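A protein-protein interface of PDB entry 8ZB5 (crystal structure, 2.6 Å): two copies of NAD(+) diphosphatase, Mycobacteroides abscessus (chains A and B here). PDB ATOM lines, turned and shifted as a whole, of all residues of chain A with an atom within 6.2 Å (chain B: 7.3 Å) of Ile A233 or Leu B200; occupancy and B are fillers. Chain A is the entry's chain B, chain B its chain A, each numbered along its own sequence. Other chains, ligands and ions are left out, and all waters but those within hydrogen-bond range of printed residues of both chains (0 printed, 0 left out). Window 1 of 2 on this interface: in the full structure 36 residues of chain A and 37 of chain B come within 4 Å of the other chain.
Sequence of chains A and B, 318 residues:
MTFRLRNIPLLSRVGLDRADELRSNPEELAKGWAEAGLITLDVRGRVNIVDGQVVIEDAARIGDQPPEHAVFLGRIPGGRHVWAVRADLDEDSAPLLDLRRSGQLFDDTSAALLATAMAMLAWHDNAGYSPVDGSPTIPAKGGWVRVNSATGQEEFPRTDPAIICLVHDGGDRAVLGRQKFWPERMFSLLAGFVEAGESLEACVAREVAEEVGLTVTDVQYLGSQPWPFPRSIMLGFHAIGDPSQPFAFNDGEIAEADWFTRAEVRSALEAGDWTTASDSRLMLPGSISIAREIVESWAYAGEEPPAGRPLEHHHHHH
OH of Tyr A221 sits at hydrogen-bond distance from OE1 of Glu B201.
The backbone NH (N) of Leu B200 sits at hydrogen-bond distance from the side-chain hydroxyl (OG) of Ser A224 (3.1 Å).
The side-chain hydroxyl (OG) of Ser A224 lies within hydrogen-bond range of the side-chain carboxylate (OE2) of Glu B201 (2.7 Å).
The backbone carbonyl oxygen (O) of Asp A160 lies within hydrogen-bond range of the backbone NH (N) of Ile A233 (2.9 Å).
O of Ala A162 lies within hydrogen-bond range of N of Leu A235.
The side-chain hydroxyl of Tyr A221 sits at hydrogen-bond distance from the side-chain hydroxyl of Ser A224 (3.2 Å).
O of Ala B162 is in hydrogen-bond range of N of Leu B235 (2.8 Å).
OE2 of Glu B198 is in hydrogen-bond range of N of Glu B195, 3.0 Å away.
The guanidinium group (NH2) of Arg B206 lies within salt-bridge range of the side-chain carboxylate (OE2) of Glu B198, at 2.7 Å.
Pro B161 touches Thr A159 (CD to O, 3.6 Å).
Tyr B221 touches Leu A200 (OH to CD1, 3.9 Å).
CD1 of Leu A200 touches CD2 of Leu B235 (3.6 Å).
Tyr A221 touches Leu B200.
Tyr A221 touches Tyr B221 (CD2 to CB, 3.3 Å).
Pro A226 touches Gly B197 (CB to C, 3.6 Å).
Pro A226 touches Glu B198.
Pro A226 touches Ser B199 (CD to N, 3.8 Å).
Ile A233 touches Leu B200.
Leu B200 touches Leu A235.
Of the printed residues of chain B, Ile A233 touches Glu B198 and Leu B200.
Printed residues of chain B within 4 Å of Leu A235: Leu B200 (3.5 Å).
Leu B200 touches just these residues of chain A: Tyr A221, Ser A224, Ile A233 and Leu A235.
Of the printed residues of chain A, Leu B235 touches Leu A200.
The nearest printed residue of chain B that does not touch Ile A233 is Val B194 (4.01 Å).
Of the 16 printed residues of chain A, 7 touch a printed residue of chain B.
Hydrophobic or aromatic side chains of chain A within 4 Å of the printed part of chain B: Leu A200, Tyr A221, Pro A226, Ile A233 and Leu A235.
Along chain A the printed residues that touch a printed residue of chain B span positions 159 to 235.
Of the 20 printed residues of chain B, 8 touch a printed residue of chain A.
Among the printed residues, 15 pairs touch across the chains.
Among the printed residues, no Asp or Glu carboxylate lies within 4 Å of a Lys or Arg side-chain nitrogen of the other chain.
Leu A200 touches Tyr B221, and with the chains exchanged Tyr A221 touches Leu B200.
Leu A200 touches Leu B235, and with the chains exchanged Leu A235 touches Leu B200.
Tyr B221 touches its own counterpart, Tyr A221.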
ATOM      1  N   THR A 159      37.314 -14.486  11.676  1.00  0.00           N
ATOM      2  CA  THR A 159      36.922 -15.815  11.262  1.00  0.00           C
ATOM      3  C   THR A 159      36.943 -15.812   9.743  1.00  0.00           C
ATOM      4  O   THR A 159      36.240 -15.015   9.142  1.00  0.00           O
ATOM      5  CB  THR A 159      35.540 -16.119  11.828  1.00  0.00           C
ATOM      6  OG1 THR A 159      35.619 -15.737  13.198  1.00  0.00           O
ATOM      7  CG2 THR A 159      35.173 -17.588  11.717  1.00  0.00           C
ATOM      8  N   ASP A 160      37.797 -16.646   9.143  1.00  0.00           N
ATOM      9  CA  ASP A 160      37.890 -16.747   7.697  1.00  0.00           C
ATOM     10  C   ASP A 160      36.893 -17.785   7.207  1.00  0.00           C
ATOM     11  O   ASP A 160      36.915 -18.921   7.667  1.00  0.00           O
ATOM     12  CB  ASP A 160      39.283 -17.139   7.241  1.00  0.00           C
ATOM     13  CG  ASP A 160      40.383 -16.147   7.576  1.00  0.00           C
ATOM     14  OD1 ASP A 160      40.034 -15.053   8.055  1.00  0.00           O
ATOM     15  OD2 ASP A 160      41.568 -16.482   7.362  1.00  0.00           O
ATOM     16  N   PRO A 161      35.967 -17.434   6.291  1.00  0.00           N
ATOM     17  CA  PRO A 161      35.057 -18.423   5.723  1.00  0.00           C
ATOM     18  C   PRO A 161      35.792 -19.259   4.687  1.00  0.00           C
ATOM     19  O   PRO A 161      36.558 -18.722   3.896  1.00  0.00           O
ATOM     20  CB  PRO A 161      33.926 -17.622   5.092  1.00  0.00           C
ATOM     21  CG  PRO A 161      34.254 -16.167   5.397  1.00  0.00           C
ATOM     22  CD  PRO A 161      35.715 -16.081   5.783  1.00  0.00           C
ATOM     23  N   ALA A 162      35.554 -20.576   4.741  1.00  0.00           N
ATOM     24  CA  ALA A 162      36.060 -21.512   3.757  1.00  0.00           C
ATOM     25  C   ALA A 162      34.912 -22.405   3.301  1.00  0.00           C
ATOM     26  O   ALA A 162      34.004 -22.700   4.075  1.00  0.00           O
ATOM     27  CB  ALA A 162      37.180 -22.318   4.353  1.00  0.00           C
ATOM     28  N   ILE A 163      34.956 -22.810   2.031  1.00  0.00           N
ATOM     29  CA  ILE A 163      33.968 -23.736   1.511  1.00  0.00           C
ATOM     30  C   ILE A 163      34.605 -25.118   1.466  1.00  0.00           C
ATOM     31  O   ILE A 163      35.822 -25.243   1.313  1.00  0.00           O
ATOM     32  CB  ILE A 163      33.411 -23.303   0.137  1.00  0.00           C
ATOM     33  CG1 ILE A 163      34.459 -23.318  -0.973  1.00  0.00           C
ATOM     34  CG2 ILE A 163      32.720 -21.944   0.231  1.00  0.00           C
ATOM     35  CD1 ILE A 163      34.702 -24.686  -1.588  1.00  0.00           C
ATOM     36  N   LEU A 200      29.560 -17.353  -2.141  1.00  0.00           N
ATOM     37  CA  LEU A 200      29.994 -18.695  -1.783  1.00  0.00           C
ATOM     38  C   LEU A 200      29.879 -19.606  -3.002  1.00  0.00           C
ATOM     39  O   LEU A 200      30.749 -20.436  -3.252  1.00  0.00           O
ATOM     40  CB  LEU A 200      29.175 -19.233  -0.612  1.00  0.00           C
ATOM     41  CG  LEU A 200      29.257 -18.443   0.697  1.00  0.00           C
ATOM     42  CD1 LEU A 200      28.442 -19.183   1.730  1.00  0.00           C
ATOM     43  CD2 LEU A 200      30.678 -18.227   1.179  1.00  0.00           C
ATOM     44  N   TYR A 221      24.088 -25.431  -0.457  1.00  0.00           N
ATOM     45  CA  TYR A 221      24.581 -25.431   0.910  1.00  0.00           C
ATOM     46  C   TYR A 221      23.990 -26.600   1.688  1.00  0.00           C
ATOM     47  O   TYR A 221      22.806 -26.883   1.564  1.00  0.00           O
ATOM     48  CB  TYR A 221      24.161 -24.087   1.522  1.00  0.00           C
ATOM     49  CG  TYR A 221      24.441 -23.892   3.008  1.00  0.00           C
ATOM     50  CD1 TYR A 221      25.685 -23.470   3.457  1.00  0.00           C
ATOM     51  CD2 TYR A 221      23.438 -24.070   3.954  1.00  0.00           C
ATOM     52  CE1 TYR A 221      25.934 -23.260   4.804  1.00  0.00           C
ATOM     53  CE2 TYR A 221      23.675 -23.870   5.304  1.00  0.00           C
ATOM     54  CZ  TYR A 221      24.929 -23.467   5.730  1.00  0.00           C
ATOM     55  OH  TYR A 221      25.201 -23.276   7.055  1.00  0.00           O
ATOM     56  N   SER A 224      27.106 -25.755   8.166  1.00  0.00           N
ATOM     57  CA  SER A 224      28.299 -25.018   8.550  1.00  0.00           C
ATOM     58  C   SER A 224      28.882 -25.558   9.848  1.00  0.00           C
ATOM     59  O   SER A 224      28.182 -26.214  10.602  1.00  0.00           O
ATOM     60  CB  SER A 224      27.984 -23.567   8.716  1.00  0.00           C
ATOM     61  OG  SER A 224      26.989 -23.407   9.716  1.00  0.00           O
ATOM     62  N   GLN A 225      30.138 -25.201  10.126  1.00  0.00           N
ATOM     63  CA  GLN A 225      30.849 -25.688  11.292  1.00  0.00           C
ATOM     64  C   GLN A 225      31.974 -24.734  11.688  1.00  0.00           C
ATOM     65  O   GLN A 225      32.877 -24.488  10.891  1.00  0.00           O
ATOM     66  CB  GLN A 225      31.483 -27.036  10.967  1.00  0.00           C
ATOM     67  CG  GLN A 225      32.123 -27.710  12.175  1.00  0.00           C
ATOM     68  CD  GLN A 225      32.839 -28.998  11.832  1.00  0.00           C
ATOM     69  OE1 GLN A 225      33.586 -29.079  10.850  1.00  0.00           O
ATOM     70  NE2 GLN A 225      32.617 -30.015  12.648  1.00  0.00           N
ATOM     71  N   PRO A 226      32.016 -24.255  12.955  1.00  0.00           N
ATOM     72  CA  PRO A 226      33.137 -23.450  13.429  1.00  0.00           C
ATOM     73  C   PRO A 226      34.375 -24.327  13.382  1.00  0.00           C
ATOM     74  O   PRO A 226      34.263 -25.508  13.685  1.00  0.00           O
ATOM     75  CB  PRO A 226      32.743 -23.039  14.856  1.00  0.00           C
ATOM     76  CG  PRO A 226      31.710 -24.066  15.278  1.00  0.00           C
ATOM     77  CD  PRO A 226      31.002 -24.484  14.003  1.00  0.00           C
ATOM     78  N   TRP A 227      35.520 -23.754  12.978  1.00  0.00           N
ATOM     79  CA  TRP A 227      36.718 -24.539  12.720  1.00  0.00           C
ATOM     80  C   TRP A 227      37.958 -23.799  13.221  1.00  0.00           C
ATOM     81  O   TRP A 227      38.821 -23.388  12.444  1.00  0.00           O
ATOM     82  CB  TRP A 227      36.830 -24.891  11.230  1.00  0.00           C
ATOM     83  CG  TRP A 227      37.701 -26.093  10.957  1.00  0.00           C
ATOM     84  CD1 TRP A 227      38.884 -26.132  10.275  1.00  0.00           C
ATOM     85  CD2 TRP A 227      37.463 -27.445  11.404  1.00  0.00           C
ATOM     86  NE1 TRP A 227      39.389 -27.405  10.253  1.00  0.00           N
ATOM     87  CE2 TRP A 227      38.539 -28.232  10.938  1.00  0.00           C
ATOM     88  CE3 TRP A 227      36.449 -28.057  12.147  1.00  0.00           C
ATOM     89  CZ2 TRP A 227      38.619 -29.596  11.186  1.00  0.00           C
ATOM     90  CZ3 TRP A 227      36.539 -29.404  12.404  1.00  0.00           C
ATOM     91  CH2 TRP A 227      37.597 -30.161  11.913  1.00  0.00           C
ATOM     92  N   ARG A 231      41.355 -20.433  12.785  1.00  0.00           N
ATOM     93  CA  ARG A 231      40.299 -19.434  12.730  1.00  0.00           C
ATOM     94  C   ARG A 231      39.456 -19.510  11.458  1.00  0.00           C
ATOM     95  O   ARG A 231      39.252 -18.498  10.795  1.00  0.00           O
ATOM     96  CB  ARG A 231      40.995 -18.074  12.775  1.00  0.00           C
ATOM     97  CG  ARG A 231      42.038 -17.933  11.675  1.00  0.00           C
ATOM     98  CD  ARG A 231      42.291 -16.487  11.371  1.00  0.00           C
ATOM     99  NE  ARG A 231      43.011 -16.266  10.115  1.00  0.00           N
ATOM    100  CZ  ARG A 231      43.950 -15.346   9.967  1.00  0.00           C
ATOM    101  NH1 ARG A 231      44.430 -14.750  11.048  1.00  0.00           N
ATOM    102  NH2 ARG A 231      44.419 -15.048   8.759  1.00  0.00           N
ATOM    103  N   SER A 232      38.943 -20.699  11.136  1.00  0.00           N
ATOM    104  CA  SER A 232      38.072 -20.864   9.987  1.00  0.00           C
ATOM    105  C   SER A 232      36.638 -21.020  10.456  1.00  0.00           C
ATOM    106  O   SER A 232      36.392 -21.204  11.644  1.00  0.00           O
ATOM    107  CB  SER A 232      38.493 -22.029   9.146  1.00  0.00           C
ATOM    108  OG  SER A 232      39.624 -21.695   8.355  1.00  0.00           O
ATOM    109  N   ILE A 233      35.707 -20.842   9.513  1.00  0.00           N
ATOM    110  CA  ILE A 233      34.367 -21.400   9.615  1.00  0.00           C
ATOM    111  C   ILE A 233      34.128 -22.094   8.290  1.00  0.00           C
ATOM    112  O   ILE A 233      34.360 -21.488   7.246  1.00  0.00           O
ATOM    113  CB  ILE A 233      33.255 -20.381   9.916  1.00  0.00           C
ATOM    114  CG1 ILE A 233      31.903 -21.056   9.928  1.00  0.00           C
ATOM    115  CG2 ILE A 233      33.247 -19.213   8.939  1.00  0.00           C
ATOM    116  CD1 ILE A 233      30.782 -20.130  10.362  1.00  0.00           C
ATOM    117  N   MET A 234      33.727 -23.370   8.364  1.00  0.00           N
ATOM    118  CA  MET A 234      33.601 -24.213   7.189  1.00  0.00           C
ATOM    119  C   MET A 234      32.146 -24.198   6.760  1.00  0.00           C
ATOM    120  O   MET A 234      31.265 -24.397   7.589  1.00  0.00           O
ATOM    121  CB  MET A 234      33.997 -25.665   7.477  1.00  0.00           C
ATOM    122  CG  MET A 234      35.438 -25.831   7.928  1.00  0.00           C
ATOM    123  SD  MET A 234      36.677 -25.343   6.716  1.00  0.00           S
ATOM    124  CE  MET A 234      35.988 -26.124   5.246  1.00  0.00           C
ATOM    125  N   LEU A 235      31.917 -23.945   5.471  1.00  0.00           N
ATOM    126  CA  LEU A 235      30.579 -23.939   4.909  1.00  0.00           C
ATOM    127  C   LEU A 235      30.509 -25.065   3.887  1.00  0.00           C
ATOM    128  O   LEU A 235      31.289 -25.073   2.942  1.00  0.00           O
ATOM    129  CB  LEU A 235      30.344 -22.564   4.305  1.00  0.00           C
ATOM    130  CG  LEU A 235      30.683 -21.405   5.246  1.00  0.00           C
ATOM    131  CD1 LEU A 235      30.657 -20.067   4.531  1.00  0.00           C
ATOM    132  CD2 LEU A 235      29.704 -21.433   6.412  1.00  0.00           C
ATOM    133  N   PRO B 161      32.184 -12.738   7.642  1.00  0.00           N
ATOM    134  CA  PRO B 161      30.837 -13.222   7.350  1.00  0.00           C
ATOM    135  C   PRO B 161      29.815 -12.558   8.260  1.00  0.00           C
ATOM    136  O   PRO B 161      30.058 -12.404   9.452  1.00  0.00           O
ATOM    137  CB  PRO B 161      30.959 -14.719   7.607  1.00  0.00           C
ATOM    138  CG  PRO B 161      32.017 -14.818   8.679  1.00  0.00           C
ATOM    139  CD  PRO B 161      33.001 -13.713   8.372  1.00  0.00           C
ATOM    140  N   ALA B 162      28.671 -12.191   7.677  1.00  0.00           N
ATOM    141  CA  ALA B 162      27.529 -11.690   8.421  1.00  0.00           C
ATOM    142  C   ALA B 162      26.265 -12.381   7.930  1.00  0.00           C
ATOM    143  O   ALA B 162      26.175 -12.726   6.765  1.00  0.00           O
ATOM    144  CB  ALA B 162      27.433 -10.191   8.267  1.00  0.00           C
ATOM    145  N   ILE B 163      25.317 -12.613   8.837  1.00  0.00           N
ATOM    146  CA  ILE B 163      24.065 -13.258   8.476  1.00  0.00           C
ATOM    147  C   ILE B 163      22.982 -12.193   8.411  1.00  0.00           C
ATOM    148  O   ILE B 163      23.067 -11.176   9.096  1.00  0.00           O
ATOM    149  CB  ILE B 163      23.666 -14.399   9.436  1.00  0.00           C
ATOM    150  CG1 ILE B 163      23.410 -13.915  10.866  1.00  0.00           C
ATOM    151  CG2 ILE B 163      24.687 -15.528   9.389  1.00  0.00           C
ATOM    152  CD1 ILE B 163      22.013 -13.358  11.102  1.00  0.00           C
ATOM    153  N   VAL B 194      28.956 -13.021  12.333  1.00  0.00           N
ATOM    154  CA  VAL B 194      29.233 -14.344  12.858  1.00  0.00           C
ATOM    155  C   VAL B 194      30.381 -14.228  13.845  1.00  0.00           C
ATOM    156  O   VAL B 194      31.430 -13.687  13.515  1.00  0.00           O
ATOM    157  CB  VAL B 194      29.636 -15.291  11.715  1.00  0.00           C
ATOM    158  CG1 VAL B 194      29.945 -16.686  12.230  1.00  0.00           C
ATOM    159  CG2 VAL B 194      28.587 -15.349  10.617  1.00  0.00           C
ATOM    160  N   GLU B 195      30.179 -14.730  15.058  1.00  0.00           N
ATOM    161  CA  GLU B 195      31.242 -14.736  16.046  1.00  0.00           C
ATOM    162  C   GLU B 195      32.082 -16.000  15.898  1.00  0.00           C
ATOM    163  O   GLU B 195      31.647 -16.978  15.300  1.00  0.00           O
ATOM    164  CB  GLU B 195      30.637 -14.599  17.437  1.00  0.00           C
ATOM    165  CG  GLU B 195      30.027 -13.218  17.633  1.00  0.00           C
ATOM    166  CD  GLU B 195      29.563 -12.891  19.033  1.00  0.00           C
ATOM    167  OE1 GLU B 195      29.167 -11.723  19.218  1.00  0.00           O
ATOM    168  OE2 GLU B 195      29.560 -13.786  19.900  1.00  0.00           O
ATOM    169  N   GLY B 197      33.519 -19.461  16.887  1.00  0.00           N
ATOM    170  CA  GLY B 197      33.087 -20.578  17.712  1.00  0.00           C
ATOM    171  C   GLY B 197      31.614 -20.944  17.531  1.00  0.00           C
ATOM    172  O   GLY B 197      31.109 -21.830  18.228  1.00  0.00           O
ATOM    173  N   GLU B 198      30.924 -20.280  16.592  1.00  0.00           N
ATOM    174  CA  GLU B 198      29.539 -20.618  16.294  1.00  0.00           C
ATOM    175  C   GLU B 198      29.381 -20.871  14.797  1.00  0.00           C
ATOM    176  O   GLU B 198      30.142 -20.353  13.986  1.00  0.00           O
ATOM    177  CB  GLU B 198      28.550 -19.575  16.815  1.00  0.00           C
ATOM    178  CG  GLU B 198      28.713 -18.199  16.182  1.00  0.00           C
ATOM    179  CD  GLU B 198      27.671 -17.172  16.587  1.00  0.00           C
ATOM    180  OE1 GLU B 198      26.890 -17.433  17.536  1.00  0.00           O
ATOM    181  OE2 GLU B 198      27.653 -16.110  15.930  1.00  0.00           O
ATOM    182  N   SER B 199      28.396 -21.717  14.476  1.00  0.00           N
ATOM    183  CA  SER B 199      27.964 -21.991  13.117  1.00  0.00           C
ATOM    184  C   SER B 199      27.011 -20.890  12.659  1.00  0.00           C
ATOM    185  O   SER B 199      26.506 -20.126  13.478  1.00  0.00           O
ATOM    186  CB  SER B 199      27.287 -23.322  13.053  1.00  0.00           C
ATOM    187  OG  SER B 199      26.122 -23.302  13.867  1.00  0.00           O
ATOM    188  N   LEU B 200      26.754 -20.826  11.347  1.00  0.00           N
ATOM    189  CA  LEU B 200      25.858 -19.817  10.813  1.00  0.00           C
ATOM    190  C   LEU B 200      24.479 -19.977  11.447  1.00  0.00           C
ATOM    191  O   LEU B 200      23.834 -18.990  11.803  1.00  0.00           O
ATOM    192  CB  LEU B 200      25.778 -19.905   9.293  1.00  0.00           C
ATOM    193  CG  LEU B 200      27.073 -19.680   8.511  1.00  0.00           C
ATOM    194  CD1 LEU B 200      26.746 -19.645   7.032  1.00  0.00           C
ATOM    195  CD2 LEU B 200      27.822 -18.424   8.879  1.00  0.00           C
ATOM    196  N   GLU B 201      24.042 -21.231  11.611  1.00  0.00           N
ATOM    197  CA  GLU B 201      22.691 -21.489  12.082  1.00  0.00           C
ATOM    198  C   GLU B 201      22.536 -21.015  13.517  1.00  0.00           C
ATOM    199  O   GLU B 201      21.505 -20.458  13.869  1.00  0.00           O
ATOM    200  CB  GLU B 201      22.320 -22.959  11.905  1.00  0.00           C
ATOM    201  CG  GLU B 201      22.010 -23.306  10.451  1.00  0.00           C
ATOM    202  CD  GLU B 201      23.199 -23.471   9.518  1.00  0.00           C
ATOM    203  OE1 GLU B 201      22.955 -23.523   8.295  1.00  0.00           O
ATOM    204  OE2 GLU B 201      24.344 -23.574  10.004  1.00  0.00           O
ATOM    205  N   ALA B 202      23.569 -21.234  14.328  1.00  0.00           N
ATOM    206  CA  ALA B 202      23.569 -20.785  15.714  1.00  0.00           C
ATOM    207  C   ALA B 202      23.631 -19.259  15.786  1.00  0.00           C
ATOM    208  O   ALA B 202      23.019 -18.642  16.653  1.00  0.00           O
ATOM    209  CB  ALA B 202      24.742 -21.402  16.443  1.00  0.00           C
ATOM    210  N   CYS B 203      24.393 -18.660  14.873  1.00  0.00           N
ATOM    211  CA  CYS B 203      24.505 -17.216  14.792  1.00  0.00           C
ATOM    212  C   CYS B 203      23.138 -16.599  14.498  1.00  0.00           C
ATOM    213  O   CYS B 203      22.739 -15.631  15.148  1.00  0.00           O
ATOM    214  CB  CYS B 203      25.534 -16.833  13.738  1.00  0.00           C
ATOM    215  SG  CYS B 203      25.714 -15.045  13.521  1.00  0.00           S
ATOM    216  N   VAL B 204      22.419 -17.167  13.521  1.00  0.00           N
ATOM    217  CA  VAL B 204      21.096 -16.679  13.170  1.00  0.00           C
ATOM    218  C   VAL B 204      20.211 -16.703  14.412  1.00  0.00           C
ATOM    219  O   VAL B 204      19.653 -15.676  14.791  1.00  0.00           O
ATOM    220  CB  VAL B 204      20.452 -17.489  12.031  1.00  0.00           C
ATOM    221  CG1 VAL B 204      18.988 -17.116  11.875  1.00  0.00           C
ATOM    222  CG2 VAL B 204      21.182 -17.300  10.712  1.00  0.00           C
ATOM    223  N   ALA B 205      20.095 -17.881  15.039  1.00  0.00           N
ATOM    224  CA  ALA B 205      19.302 -18.056  16.255  1.00  0.00           C
ATOM    225  C   ALA B 205      19.731 -17.073  17.342  1.00  0.00           C
ATOM    226  O   ALA B 205      18.884 -16.480  17.994  1.00  0.00           O
ATOM    227  CB  ALA B 205      19.420 -19.473  16.757  1.00  0.00           C
ATOM    228  N   ARG B 206      21.044 -16.894  17.515  1.00  0.00           N
ATOM    229  CA  ARG B 206      21.566 -15.973  18.511  1.00  0.00           C
ATOM    230  C   ARG B 206      21.148 -14.549  18.153  1.00  0.00           C
ATOM    231  O   ARG B 206      20.593 -13.854  18.993  1.00  0.00           O
ATOM    232  CB  ARG B 206      23.094 -16.058  18.676  1.00  0.00           C
ATOM    233  CG  ARG B 206      23.680 -15.153  19.749  1.00  0.00           C
ATOM    234  CD  ARG B 206      25.190 -15.300  19.924  1.00  0.00           C
ATOM    235  NE  ARG B 206      25.927 -15.058  18.677  1.00  0.00           N
ATOM    236  CZ  ARG B 206      26.000 -13.897  18.021  1.00  0.00           C
ATOM    237  NH1 ARG B 206      25.499 -12.791  18.562  1.00  0.00           N
ATOM    238  NH2 ARG B 206      26.586 -13.840  16.828  1.00  0.00           N
ATOM    239  N   VAL B 219      16.260 -23.047  10.401  1.00  0.00           N
ATOM    240  CA  VAL B 219      17.101 -22.015   9.822  1.00  0.00           C
ATOM    241  C   VAL B 219      17.705 -22.521   8.513  1.00  0.00           C
ATOM    242  O   VAL B 219      18.499 -23.453   8.548  1.00  0.00           O
ATOM    243  CB  VAL B 219      18.182 -21.676  10.863  1.00  0.00           C
ATOM    244  CG1 VAL B 219      19.245 -20.732  10.319  1.00  0.00           C
ATOM    245  CG2 VAL B 219      17.568 -21.088  12.124  1.00  0.00           C
ATOM    246  N   TYR B 221      19.501 -21.564   4.583  1.00  0.00           N
ATOM    247  CA  TYR B 221      20.243 -20.664   3.718  1.00  0.00           C
ATOM    248  C   TYR B 221      19.493 -20.414   2.413  1.00  0.00           C
ATOM    249  O   TYR B 221      18.931 -21.333   1.834  1.00  0.00           O
ATOM    250  CB  TYR B 221      21.588 -21.339   3.449  1.00  0.00           C
ATOM    251  CG  TYR B 221      22.513 -20.662   2.450  1.00  0.00           C
ATOM    252  CD1 TYR B 221      23.364 -19.638   2.849  1.00  0.00           C
ATOM    253  CD2 TYR B 221      22.587 -21.100   1.136  1.00  0.00           C
ATOM    254  CE1 TYR B 221      24.232 -19.033   1.957  1.00  0.00           C
ATOM    255  CE2 TYR B 221      23.453 -20.504   0.232  1.00  0.00           C
ATOM    256  CZ  TYR B 221      24.276 -19.471   0.647  1.00  0.00           C
ATOM    257  OH  TYR B 221      25.129 -18.878  -0.235  1.00  0.00           O
ATOM    258  N   LEU B 235      25.275 -13.502   4.215  1.00  0.00           N
ATOM    259  CA  LEU B 235      24.719 -14.828   4.022  1.00  0.00           C
ATOM    260  C   LEU B 235      23.262 -14.780   4.436  1.00  0.00           C
ATOM    261  O   LEU B 235      22.968 -14.445   5.575  1.00  0.00           O
ATOM    262  CB  LEU B 235      25.551 -15.788   4.859  1.00  0.00           C
ATOM    263  CG  LEU B 235      27.059 -15.673   4.598  1.00  0.00           C
ATOM    264  CD1 LEU B 235      27.884 -16.489   5.556  1.00  0.00           C
ATOM    265  CD2 LEU B 235      27.344 -16.102   3.174  1.00  0.00           C
ATOM    266  N   GLY B 236      22.372 -15.061   3.478  1.00  0.00           N
ATOM    267  CA  GLY B 236      20.947 -14.882   3.692  1.00  0.00           C
ATOM    268  C   GLY B 236      20.280 -16.163   4.167  1.00  0.00           C
ATOM    269  O   GLY B 236      20.571 -17.239   3.651  1.00  0.00           O
ATOM    270  N   PHE B 237      19.374 -16.012   5.135  1.00  0.00           N
ATOM    271  CA  PHE B 237      18.676 -17.135   5.744  1.00  0.00           C
ATOM    272  C   PHE B 237      17.203 -16.796   5.943  1.00  0.00           C
ATOM    273  O   PHE B 237      16.834 -15.625   5.968  1.00  0.00           O
ATOM    274  CB  PHE B 237      19.266 -17.459   7.124  1.00  0.00           C
ATOM    275  CG  PHE B 237      20.618 -18.142   7.082  1.00  0.00           C
ATOM    276  CD1 PHE B 237      21.788 -17.403   6.993  1.00  0.00           C
ATOM    277  CD2 PHE B 237      20.711 -19.523   7.124  1.00  0.00           C
ATOM    278  CE1 PHE B 237      23.016 -18.036   6.941  1.00  0.00           C
ATOM    279  CE2 PHE B 237      21.943 -20.145   7.061  1.00  0.00           C
ATOM    280  CZ  PHE B 237      23.088 -19.403   6.966  1.00  0.00           C
